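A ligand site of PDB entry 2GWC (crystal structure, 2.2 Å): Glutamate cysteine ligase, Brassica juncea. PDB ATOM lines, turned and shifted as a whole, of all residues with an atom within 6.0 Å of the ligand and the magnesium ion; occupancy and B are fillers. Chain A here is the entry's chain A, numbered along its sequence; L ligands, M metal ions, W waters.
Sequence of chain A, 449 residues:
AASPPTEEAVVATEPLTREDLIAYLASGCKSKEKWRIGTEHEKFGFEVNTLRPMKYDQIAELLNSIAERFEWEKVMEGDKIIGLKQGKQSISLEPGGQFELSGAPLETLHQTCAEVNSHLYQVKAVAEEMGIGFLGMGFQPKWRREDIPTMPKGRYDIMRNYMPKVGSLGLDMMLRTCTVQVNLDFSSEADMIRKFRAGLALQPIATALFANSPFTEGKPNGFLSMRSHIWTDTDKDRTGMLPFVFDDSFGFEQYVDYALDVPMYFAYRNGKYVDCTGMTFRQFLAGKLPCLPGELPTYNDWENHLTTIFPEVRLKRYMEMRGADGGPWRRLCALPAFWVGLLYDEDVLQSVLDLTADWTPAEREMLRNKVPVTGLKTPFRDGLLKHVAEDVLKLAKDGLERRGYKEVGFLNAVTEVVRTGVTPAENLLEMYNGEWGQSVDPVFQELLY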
ATOM      1  N   GLU A  40       3.189   7.599  -4.026  1.00  0.00           N
ATOM      2  CA  GLU A  40       2.031   6.855  -4.546  1.00  0.00           C
ATOM      3  C   GLU A  40       1.956   5.493  -3.819  1.00  0.00           C
ATOM      4  O   GLU A  40       2.946   4.907  -3.530  1.00  0.00           O
ATOM      5  CB  GLU A  40       2.111   6.580  -6.042  1.00  0.00           C
ATOM      6  CG  GLU A  40       2.556   7.759  -6.953  1.00  0.00           C
ATOM      7  CD  GLU A  40       2.704   7.337  -8.427  1.00  0.00           C
ATOM      8  OE1 GLU A  40       2.068   6.333  -8.828  1.00  0.00           O
ATOM      9  OE2 GLU A  40       3.512   8.008  -9.168  1.00  0.00           O
ATOM     10  N   GLU A  42      -0.777   1.743  -3.569  1.00  0.00           N
ATOM     11  CA  GLU A  42      -1.940   1.005  -3.993  1.00  0.00           C
ATOM     12  C   GLU A  42      -2.381   0.052  -2.863  1.00  0.00           C
ATOM     13  O   GLU A  42      -1.541  -0.467  -2.090  1.00  0.00           O
ATOM     14  CB  GLU A  42      -1.586   0.214  -5.250  1.00  0.00           C
ATOM     15  CG  GLU A  42      -0.830   1.027  -6.346  1.00  0.00           C
ATOM     16  CD  GLU A  42      -0.127   0.190  -7.364  1.00  0.00           C
ATOM     17  OE1 GLU A  42       0.245  -0.985  -7.089  1.00  0.00           O
ATOM     18  OE2 GLU A  42       0.113   0.732  -8.471  1.00  0.00           O
ATOM     19  N   GLU A  94      -5.969   0.522 -10.400  1.00  0.00           N
ATOM     20  CA  GLU A  94      -5.128  -0.405 -11.143  1.00  0.00           C
ATOM     21  C   GLU A  94      -6.036  -1.452 -11.818  1.00  0.00           C
ATOM     22  O   GLU A  94      -7.277  -1.456 -11.599  1.00  0.00           O
ATOM     23  CB  GLU A  94      -4.074  -1.055 -10.227  1.00  0.00           C
ATOM     24  CG  GLU A  94      -3.020  -0.071  -9.731  1.00  0.00           C
ATOM     25  CD  GLU A  94      -2.024   0.363 -10.804  1.00  0.00           C
ATOM     26  OE1 GLU A  94      -1.987  -0.241 -11.864  1.00  0.00           O
ATOM     27  OE2 GLU A  94      -1.253   1.299 -10.588  1.00  0.00           O
ATOM     28  N   PRO A  95      -5.447  -2.295 -12.679  1.00  0.00           N
ATOM     29  CA  PRO A  95      -6.269  -3.243 -13.454  1.00  0.00           C
ATOM     30  C   PRO A  95      -7.181  -4.167 -12.661  1.00  0.00           C
ATOM     31  O   PRO A  95      -8.261  -4.501 -13.129  1.00  0.00           O
ATOM     32  CB  PRO A  95      -5.219  -4.040 -14.241  1.00  0.00           C
ATOM     33  CG  PRO A  95      -4.131  -3.058 -14.441  1.00  0.00           C
ATOM     34  CD  PRO A  95      -4.045  -2.364 -13.093  1.00  0.00           C
ATOM     35  N   GLN A  98      -7.191  -2.325  -7.587  1.00  0.00           N
ATOM     36  CA  GLN A  98      -6.342  -1.785  -6.523  1.00  0.00           C
ATOM     37  C   GLN A  98      -6.512  -0.260  -6.497  1.00  0.00           C
ATOM     38  O   GLN A  98      -6.488   0.406  -7.507  1.00  0.00           O
ATOM     39  CB  GLN A  98      -4.876  -2.149  -6.703  1.00  0.00           C
ATOM     40  CG  GLN A  98      -4.608  -3.649  -6.914  1.00  0.00           C
ATOM     41  CD  GLN A  98      -4.409  -4.033  -8.374  1.00  0.00           C
ATOM     42  OE1 GLN A  98      -5.279  -3.793  -9.184  1.00  0.00           O
ATOM     43  NE2 GLN A  98      -3.257  -4.616  -8.703  1.00  0.00           N
ATOM     44  N   GLU A 100      -5.591   3.366  -5.625  1.00  0.00           N
ATOM     45  CA  GLU A 100      -4.329   4.094  -5.628  1.00  0.00           C
ATOM     46  C   GLU A 100      -4.456   5.599  -5.289  1.00  0.00           C
ATOM     47  O   GLU A 100      -5.291   6.287  -5.812  1.00  0.00           O
ATOM     48  CB  GLU A 100      -3.659   3.939  -7.003  1.00  0.00           C
ATOM     49  CG  GLU A 100      -2.225   4.510  -7.025  1.00  0.00           C
ATOM     50  CD  GLU A 100      -1.579   4.515  -8.380  1.00  0.00           C
ATOM     51  OE1 GLU A 100      -1.208   3.410  -8.878  1.00  0.00           O
ATOM     52  OE2 GLU A 100      -1.393   5.623  -8.949  1.00  0.00           O
ATOM     53  N   GLY A 138       1.821  -6.732  -0.681  1.00  0.00           N
ATOM     54  CA  GLY A 138       2.402  -6.660  -2.019  1.00  0.00           C
ATOM     55  C   GLY A 138       1.740  -7.535  -3.059  1.00  0.00           C
ATOM     56  O   GLY A 138       1.817  -7.229  -4.258  1.00  0.00           O
ATOM     57  N   TYR A 156      -6.047  -0.821 -20.115  1.00  0.00           N
ATOM     58  CA  TYR A 156      -5.794  -2.115 -19.493  1.00  0.00           C
ATOM     59  C   TYR A 156      -6.250  -3.284 -20.336  1.00  0.00           C
ATOM     60  O   TYR A 156      -5.681  -4.339 -20.220  1.00  0.00           O
ATOM     61  CB  TYR A 156      -6.443  -2.197 -18.109  1.00  0.00           C
ATOM     62  CG  TYR A 156      -5.911  -1.196 -17.120  1.00  0.00           C
ATOM     63  CD1 TYR A 156      -4.681  -0.579 -17.295  1.00  0.00           C
ATOM     64  CD2 TYR A 156      -6.652  -0.880 -15.989  1.00  0.00           C
ATOM     65  CE1 TYR A 156      -4.213   0.335 -16.382  1.00  0.00           C
ATOM     66  CE2 TYR A 156      -6.157   0.022 -15.042  1.00  0.00           C
ATOM     67  CZ  TYR A 156      -4.974   0.625 -15.250  1.00  0.00           C
ATOM     68  OH  TYR A 156      -4.556   1.518 -14.316  1.00  0.00           O
ATOM     69  N   MET A 159      -3.383  -3.860 -22.664  1.00  0.00           N
ATOM     70  CA  MET A 159      -2.294  -4.450 -21.917  1.00  0.00           C
ATOM     71  C   MET A 159      -2.525  -5.900 -21.558  1.00  0.00           C
ATOM     72  O   MET A 159      -1.604  -6.701 -21.647  1.00  0.00           O
ATOM     73  CB  MET A 159      -2.003  -3.651 -20.649  1.00  0.00           C
ATOM     74  CG  MET A 159      -1.427  -2.324 -20.927  1.00  0.00           C
ATOM     75  SD  MET A 159      -1.128  -1.390 -19.202  1.00  0.00           S
ATOM     76  CE  MET A 159       0.182  -2.723 -18.291  1.00  0.00           C
ATOM     77  N   MET A 163       0.094  -8.898 -22.583  1.00  0.00           N
ATOM     78  CA  MET A 163       0.955  -9.505 -21.553  1.00  0.00           C
ATOM     79  C   MET A 163       1.364 -10.964 -21.799  1.00  0.00           C
ATOM     80  O   MET A 163       2.533 -11.312 -21.585  1.00  0.00           O
ATOM     81  CB  MET A 163       0.308  -9.410 -20.172  1.00  0.00           C
ATOM     82  CG  MET A 163       0.463  -8.083 -19.564  1.00  0.00           C
ATOM     83  SD  MET A 163       2.321  -7.416 -19.308  1.00  0.00           S
ATOM     84  CE  MET A 163       1.852  -5.556 -18.666  1.00  0.00           C
ATOM     85  N   MET A 173       1.081  -9.217 -12.257  1.00  0.00           N
ATOM     86  CA  MET A 173       1.495  -7.842 -11.982  1.00  0.00           C
ATOM     87  C   MET A 173       0.272  -6.889 -12.029  1.00  0.00           C
ATOM     88  O   MET A 173       0.029  -6.125 -11.107  1.00  0.00           O
ATOM     89  CB  MET A 173       2.586  -7.403 -12.981  1.00  0.00           C
ATOM     90  CG  MET A 173       3.139  -6.001 -12.774  1.00  0.00           C
ATOM     91  SD  MET A 173       1.959  -4.550 -13.523  1.00  0.00           S
ATOM     92  CE  MET A 173       2.357  -4.830 -15.504  1.00  0.00           C
ATOM     93  N   MET A 174      -0.493  -6.979 -13.102  1.00  0.00           N
ATOM     94  CA  MET A 174      -1.636  -6.081 -13.324  1.00  0.00           C
ATOM     95  C   MET A 174      -2.771  -6.241 -12.300  1.00  0.00           C
ATOM     96  O   MET A 174      -3.286  -5.241 -11.760  1.00  0.00           O
ATOM     97  CB  MET A 174      -2.208  -6.294 -14.733  1.00  0.00           C
ATOM     98  CG  MET A 174      -1.264  -5.820 -15.839  1.00  0.00           C
ATOM     99  SD  MET A 174      -2.033  -6.174 -17.614  1.00  0.00           S
ATOM    100  CE  MET A 174      -3.429  -4.723 -17.617  1.00  0.00           C
ATOM    101  N   THR A 177      -0.930  -7.339  -7.680  1.00  0.00           N
ATOM    102  CA  THR A 177       0.179  -6.710  -6.946  1.00  0.00           C
ATOM    103  C   THR A 177      -0.157  -5.309  -6.463  1.00  0.00           C
ATOM    104  O   THR A 177      -0.960  -4.642  -7.103  1.00  0.00           O
ATOM    105  CB  THR A 177       1.464  -6.573  -7.807  1.00  0.00           C
ATOM    106  OG1 THR A 177       1.178  -5.779  -8.979  1.00  0.00           O
ATOM    107  CG2 THR A 177       2.017  -7.937  -8.159  1.00  0.00           C
ATOM    108  N   CYS A 178       0.467  -4.883  -5.360  1.00  0.00           N
ATOM    109  CA  CYS A 178       0.381  -3.510  -4.845  1.00  0.00           C
ATOM    110  C   CYS A 178       1.746  -3.005  -4.409  1.00  0.00           C
ATOM    111  O   CYS A 178       2.520  -3.720  -3.739  1.00  0.00           O
ATOM    112  CB  CYS A 178      -0.574  -3.392  -3.631  1.00  0.00           C
ATOM    113  SG  CYS A 178      -2.321  -3.317  -4.002  1.00  0.00           S
ATOM    114  N   THR A 179       2.033  -1.758  -4.763  1.00  0.00           N
ATOM    115  CA  THR A 179       3.325  -1.125  -4.484  1.00  0.00           C
ATOM    116  C   THR A 179       3.142   0.147  -3.633  1.00  0.00           C
ATOM    117  O   THR A 179       2.066   0.737  -3.610  1.00  0.00           O
ATOM    118  CB  THR A 179       4.087  -0.735  -5.815  1.00  0.00           C
ATOM    119  OG1 THR A 179       5.320  -0.071  -5.506  1.00  0.00           O
ATOM    120  CG2 THR A 179       3.317   0.212  -6.636  1.00  0.00           C
ATOM    121  N   GLN A 181       5.437   3.631  -3.858  1.00  0.00           N
ATOM    122  CA  GLN A 181       6.572   4.279  -4.533  1.00  0.00           C
ATOM    123  C   GLN A 181       6.775   5.747  -4.171  1.00  0.00           C
ATOM    124  O   GLN A 181       5.889   6.379  -3.603  1.00  0.00           O
ATOM    125  CB  GLN A 181       6.455   4.138  -6.023  1.00  0.00           C
ATOM    126  CG  GLN A 181       5.318   4.797  -6.657  1.00  0.00           C
ATOM    127  CD  GLN A 181       5.498   4.716  -8.156  1.00  0.00           C
ATOM    128  OE1 GLN A 181       5.313   3.634  -8.745  1.00  0.00           O
ATOM    129  NE2 GLN A 181       5.883   5.844  -8.779  1.00  0.00           N
ATOM    130  N   ARG A 227       5.665 -10.412  -5.407  1.00  0.00           N
ATOM    131  CA  ARG A 227       5.479  -9.246  -6.258  1.00  0.00           C
ATOM    132  C   ARG A 227       6.751  -8.868  -7.037  1.00  0.00           C
ATOM    133  O   ARG A 227       6.680  -8.660  -8.229  1.00  0.00           O
ATOM    134  CB  ARG A 227       5.033  -8.057  -5.439  1.00  0.00           C
ATOM    135  CG  ARG A 227       5.071  -6.725  -6.183  1.00  0.00           C
ATOM    136  CD  ARG A 227       4.778  -5.556  -5.233  1.00  0.00           C
ATOM    137  NE  ARG A 227       5.190  -4.347  -5.883  1.00  0.00           N
ATOM    138  CZ  ARG A 227       6.437  -3.895  -5.905  1.00  0.00           C
ATOM    139  NH1 ARG A 227       7.404  -4.477  -5.211  1.00  0.00           N
ATOM    140  NH2 ARG A 227       6.719  -2.820  -6.619  1.00  0.00           N
ATOM    141  N   TRP A 231       7.718  -9.206 -11.361  1.00  0.00           N
ATOM    142  CA  TRP A 231       8.345  -8.236 -12.245  1.00  0.00           C
ATOM    143  C   TRP A 231       9.525  -8.738 -13.060  1.00  0.00           C
ATOM    144  O   TRP A 231       9.963  -8.019 -13.962  1.00  0.00           O
ATOM    145  CB  TRP A 231       8.760  -6.998 -11.439  1.00  0.00           C
ATOM    146  CG  TRP A 231       7.636  -6.049 -11.159  1.00  0.00           C
ATOM    147  CD1 TRP A 231       7.049  -5.807  -9.941  1.00  0.00           C
ATOM    148  CD2 TRP A 231       6.952  -5.199 -12.100  1.00  0.00           C
ATOM    149  NE1 TRP A 231       6.064  -4.861 -10.070  1.00  0.00           N
ATOM    150  CE2 TRP A 231       6.008  -4.440 -11.377  1.00  0.00           C
ATOM    151  CE3 TRP A 231       7.082  -4.962 -13.475  1.00  0.00           C
ATOM    152  CZ2 TRP A 231       5.174  -3.497 -11.997  1.00  0.00           C
ATOM    153  CZ3 TRP A 231       6.280  -4.040 -14.082  1.00  0.00           C
ATOM    154  CH2 TRP A 231       5.327  -3.323 -13.344  1.00  0.00           C
ATOM    155  N   THR A 307       5.430   6.422 -19.306  1.00  0.00           N
ATOM    156  CA  THR A 307       4.675   5.817 -18.211  1.00  0.00           C
ATOM    157  C   THR A 307       4.343   4.330 -18.445  1.00  0.00           C
ATOM    158  O   THR A 307       3.777   3.679 -17.563  1.00  0.00           O
ATOM    159  CB  THR A 307       3.373   6.639 -17.960  1.00  0.00           C
ATOM    160  OG1 THR A 307       3.734   8.002 -17.784  1.00  0.00           O
ATOM    161  CG2 THR A 307       2.625   6.217 -16.711  1.00  0.00           C
ATOM    162  N   PHE A 310       8.739   0.126 -17.157  1.00  0.00           N
ATOM    163  CA  PHE A 310       8.647  -0.376 -15.754  1.00  0.00           C
ATOM    164  C   PHE A 310       9.949  -0.907 -15.140  1.00  0.00           C
ATOM    165  O   PHE A 310       9.985  -2.003 -14.550  1.00  0.00           O
ATOM    166  CB  PHE A 310       7.564  -1.460 -15.645  1.00  0.00           C
ATOM    167  CG  PHE A 310       6.212  -1.040 -16.199  1.00  0.00           C
ATOM    168  CD1 PHE A 310       5.591   0.115 -15.743  1.00  0.00           C
ATOM    169  CD2 PHE A 310       5.590  -1.788 -17.183  1.00  0.00           C
ATOM    170  CE1 PHE A 310       4.313   0.518 -16.243  1.00  0.00           C
ATOM    171  CE2 PHE A 310       4.342  -1.391 -17.704  1.00  0.00           C
ATOM    172  CZ  PHE A 310       3.700  -0.233 -17.224  1.00  0.00           C
ATOM    173  N   ARG A 314      12.659   4.330 -12.535  1.00  0.00           N
ATOM    174  CA  ARG A 314      12.195   4.932 -13.784  1.00  0.00           C
ATOM    175  C   ARG A 314      12.550   6.421 -13.868  1.00  0.00           C
ATOM    176  O   ARG A 314      12.553   7.126 -12.852  1.00  0.00           O
ATOM    177  CB  ARG A 314      10.695   4.741 -13.873  1.00  0.00           C
ATOM    178  CG  ARG A 314      10.059   5.210 -15.192  1.00  0.00           C
ATOM    179  CD  ARG A 314       8.627   5.643 -14.906  1.00  0.00           C
ATOM    180  NE  ARG A 314       7.744   4.583 -15.276  1.00  0.00           N
ATOM    181  CZ  ARG A 314       6.435   4.562 -15.044  1.00  0.00           C
ATOM    182  NH1 ARG A 314       5.812   5.525 -14.357  1.00  0.00           N
ATOM    183  NH2 ARG A 314       5.775   3.507 -15.479  1.00  0.00           N
ATOM    184  N   ARG A 322      10.677   2.154  -7.632  1.00  0.00           N
ATOM    185  CA  ARG A 322       9.518   1.260  -7.865  1.00  0.00           C
ATOM    186  C   ARG A 322       9.616  -0.143  -7.228  1.00  0.00           C
ATOM    187  O   ARG A 322       8.779  -0.991  -7.491  1.00  0.00           O
ATOM    188  CB  ARG A 322       9.290   1.140  -9.370  1.00  0.00           C
ATOM    189  CG  ARG A 322       8.988   2.450 -10.078  1.00  0.00           C
ATOM    190  CD  ARG A 322       8.990   2.270 -11.583  1.00  0.00           C
ATOM    191  NE  ARG A 322       8.234   1.099 -11.990  1.00  0.00           N
ATOM    192  CZ  ARG A 322       6.906   1.035 -12.172  1.00  0.00           C
ATOM    193  NH1 ARG A 322       6.120   2.079 -12.056  1.00  0.00           N
ATOM    194  NH2 ARG A 322       6.387  -0.120 -12.539  1.00  0.00           N
ATOM    195  N   ALA A 324       9.401  -1.451  -3.969  1.00  0.00           N
ATOM    196  CA  ALA A 324       8.824  -1.832  -2.665  1.00  0.00           C
ATOM    197  C   ALA A 324       7.357  -2.261  -2.695  1.00  0.00           C
ATOM    198  O   ALA A 324       6.517  -1.624  -3.353  1.00  0.00           O
ATOM    199  CB  ALA A 324       8.976  -0.693  -1.662  1.00  0.00           C
HETATM  200  C1  LIG L   1      -1.057  -1.211 -14.986  1.00  0.00           C
HETATM  201  C2  LIG L   1       0.458  -1.388 -14.842  1.00  0.00           C
HETATM  202  C3  LIG L   1       1.241  -0.095 -14.724  1.00  0.00           C
HETATM  203  C4  LIG L   1       1.002   0.682 -13.428  1.00  0.00           C
HETATM  204  S1  LIG L   1       2.190   0.396 -12.066  1.00  0.00           S
HETATM  205  N1  LIG L   1       3.665   0.358 -12.600  1.00  0.00           N
HETATM  206  O1  LIG L   1       1.979   1.525 -11.125  1.00  0.00           O
HETATM  207  C5  LIG L   1       1.722  -1.106 -11.190  1.00  0.00           C
HETATM  208  C6  LIG L   1       2.404  -1.313  -9.883  1.00  0.00           C
HETATM  209  C7  LIG L   1       2.104  -2.727  -9.443  1.00  0.00           C
HETATM  210  C8  LIG L   1       3.142  -3.039  -8.388  1.00  0.00           C
HETATM  211  O2  LIG L   1       2.711  -3.553  -7.343  1.00  0.00           O
HETATM  212  O3  LIG L   1       4.327  -2.733  -8.641  1.00  0.00           O
HETATM  213  N2  LIG L   1       0.726  -2.859  -8.918  1.00  0.00           N
HETATM  214 MG    MG M   1       0.318   2.379  -9.630  1.00  0.00          MG
HETATM  215  O   HOH W   1      -0.900  -3.089 -11.119  1.00  0.00           O
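The guanidinium group (NH2) of Arg 322 sits close to a nitrogen (N1) of the ligand, 2.8 Å away. The guanidinium group (NE) of Arg 227 is in salt-bridge range of an oxygen (O2) of the ligand, at 3.0 Å. The backbone carbonyl oxygen of Thr 177 is in hydrogen-bond range of a nitrogen (N2) of the ligand (3.1 Å). The backbone NH of Cys 178 lies close to an oxygen (O2) of the ligand. O2 of the ligand is in hydrogen-bond range of N of Thr 179. The side-chain hydroxyl (OG1) of Thr 177 lies within hydrogen-bond range of a nitrogen (N2) of the ligand (3.0 Å). NE1 of Trp 231 sits at hydrogen-bond distance from O3 of the ligand (3.1 Å).
The backbone carbonyl oxygen (O) of Glu 42 sits close to the side-chain sulfur (SG) of Cys 178 (3.5 Å). The side-chain amide nitrogen (NE2) of Gln 98 is in hydrogen-bond range of the backbone carbonyl oxygen (O) of Thr 177 (2.8 Å). O of Met 173 sits at hydrogen-bond distance from OG1 of Thr 177, at 2.4 Å. NE of Arg 227 sits close to O of Cys 178 (3.5 Å). The backbone NH (N) of Glu 42 sits at hydrogen-bond distance from the backbone carbonyl oxygen (O) of Thr 179, 3.0 Å away. NH2 of Arg 227 sits close to O of Ala 324 (3.5 Å). The side-chain hydroxyl (OG1) of Thr 179 sits at hydrogen-bond distance from the backbone carbonyl oxygen (O) of Ala 324, at 2.9 Å. The side-chain hydroxyl (OG1) of Thr 179 sits at hydrogen-bond distance from the guanidinium group (NH2) of Arg 227, at 3.3 Å.
Residues that only touch the ligand: Pro 95, Tyr 156, Met 159, Met 173 and Phe 310. Hydrophobic or aromatic side chains within 4 Å of the ligand: Pro 95, Tyr 156, Met 159, Met 173, Trp 231 and Phe 310. Of the 23 residues printed, 13 come within 4 Å of the ligand.
Within 4 Å of the magnesium ion: Glu 42, Glu 94 and Glu 100. Along chain A the residues within 4 Å of the magnesium ion span positions 42 to 100. The nearest printed residue that does not touch the magnesium ion is Glu 40 (4.4 Å).
The magnesium ion is bound by the side-chain carboxylate (OE1) of Glu 100 (2.0 Å), the side-chain carboxylate (OE2) of Glu 42 (2.0 Å), the side-chain carboxylate (OE2) of Glu 94 (2.1 Å) and an oxygen (O1) of the ligand (2.4 Å).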
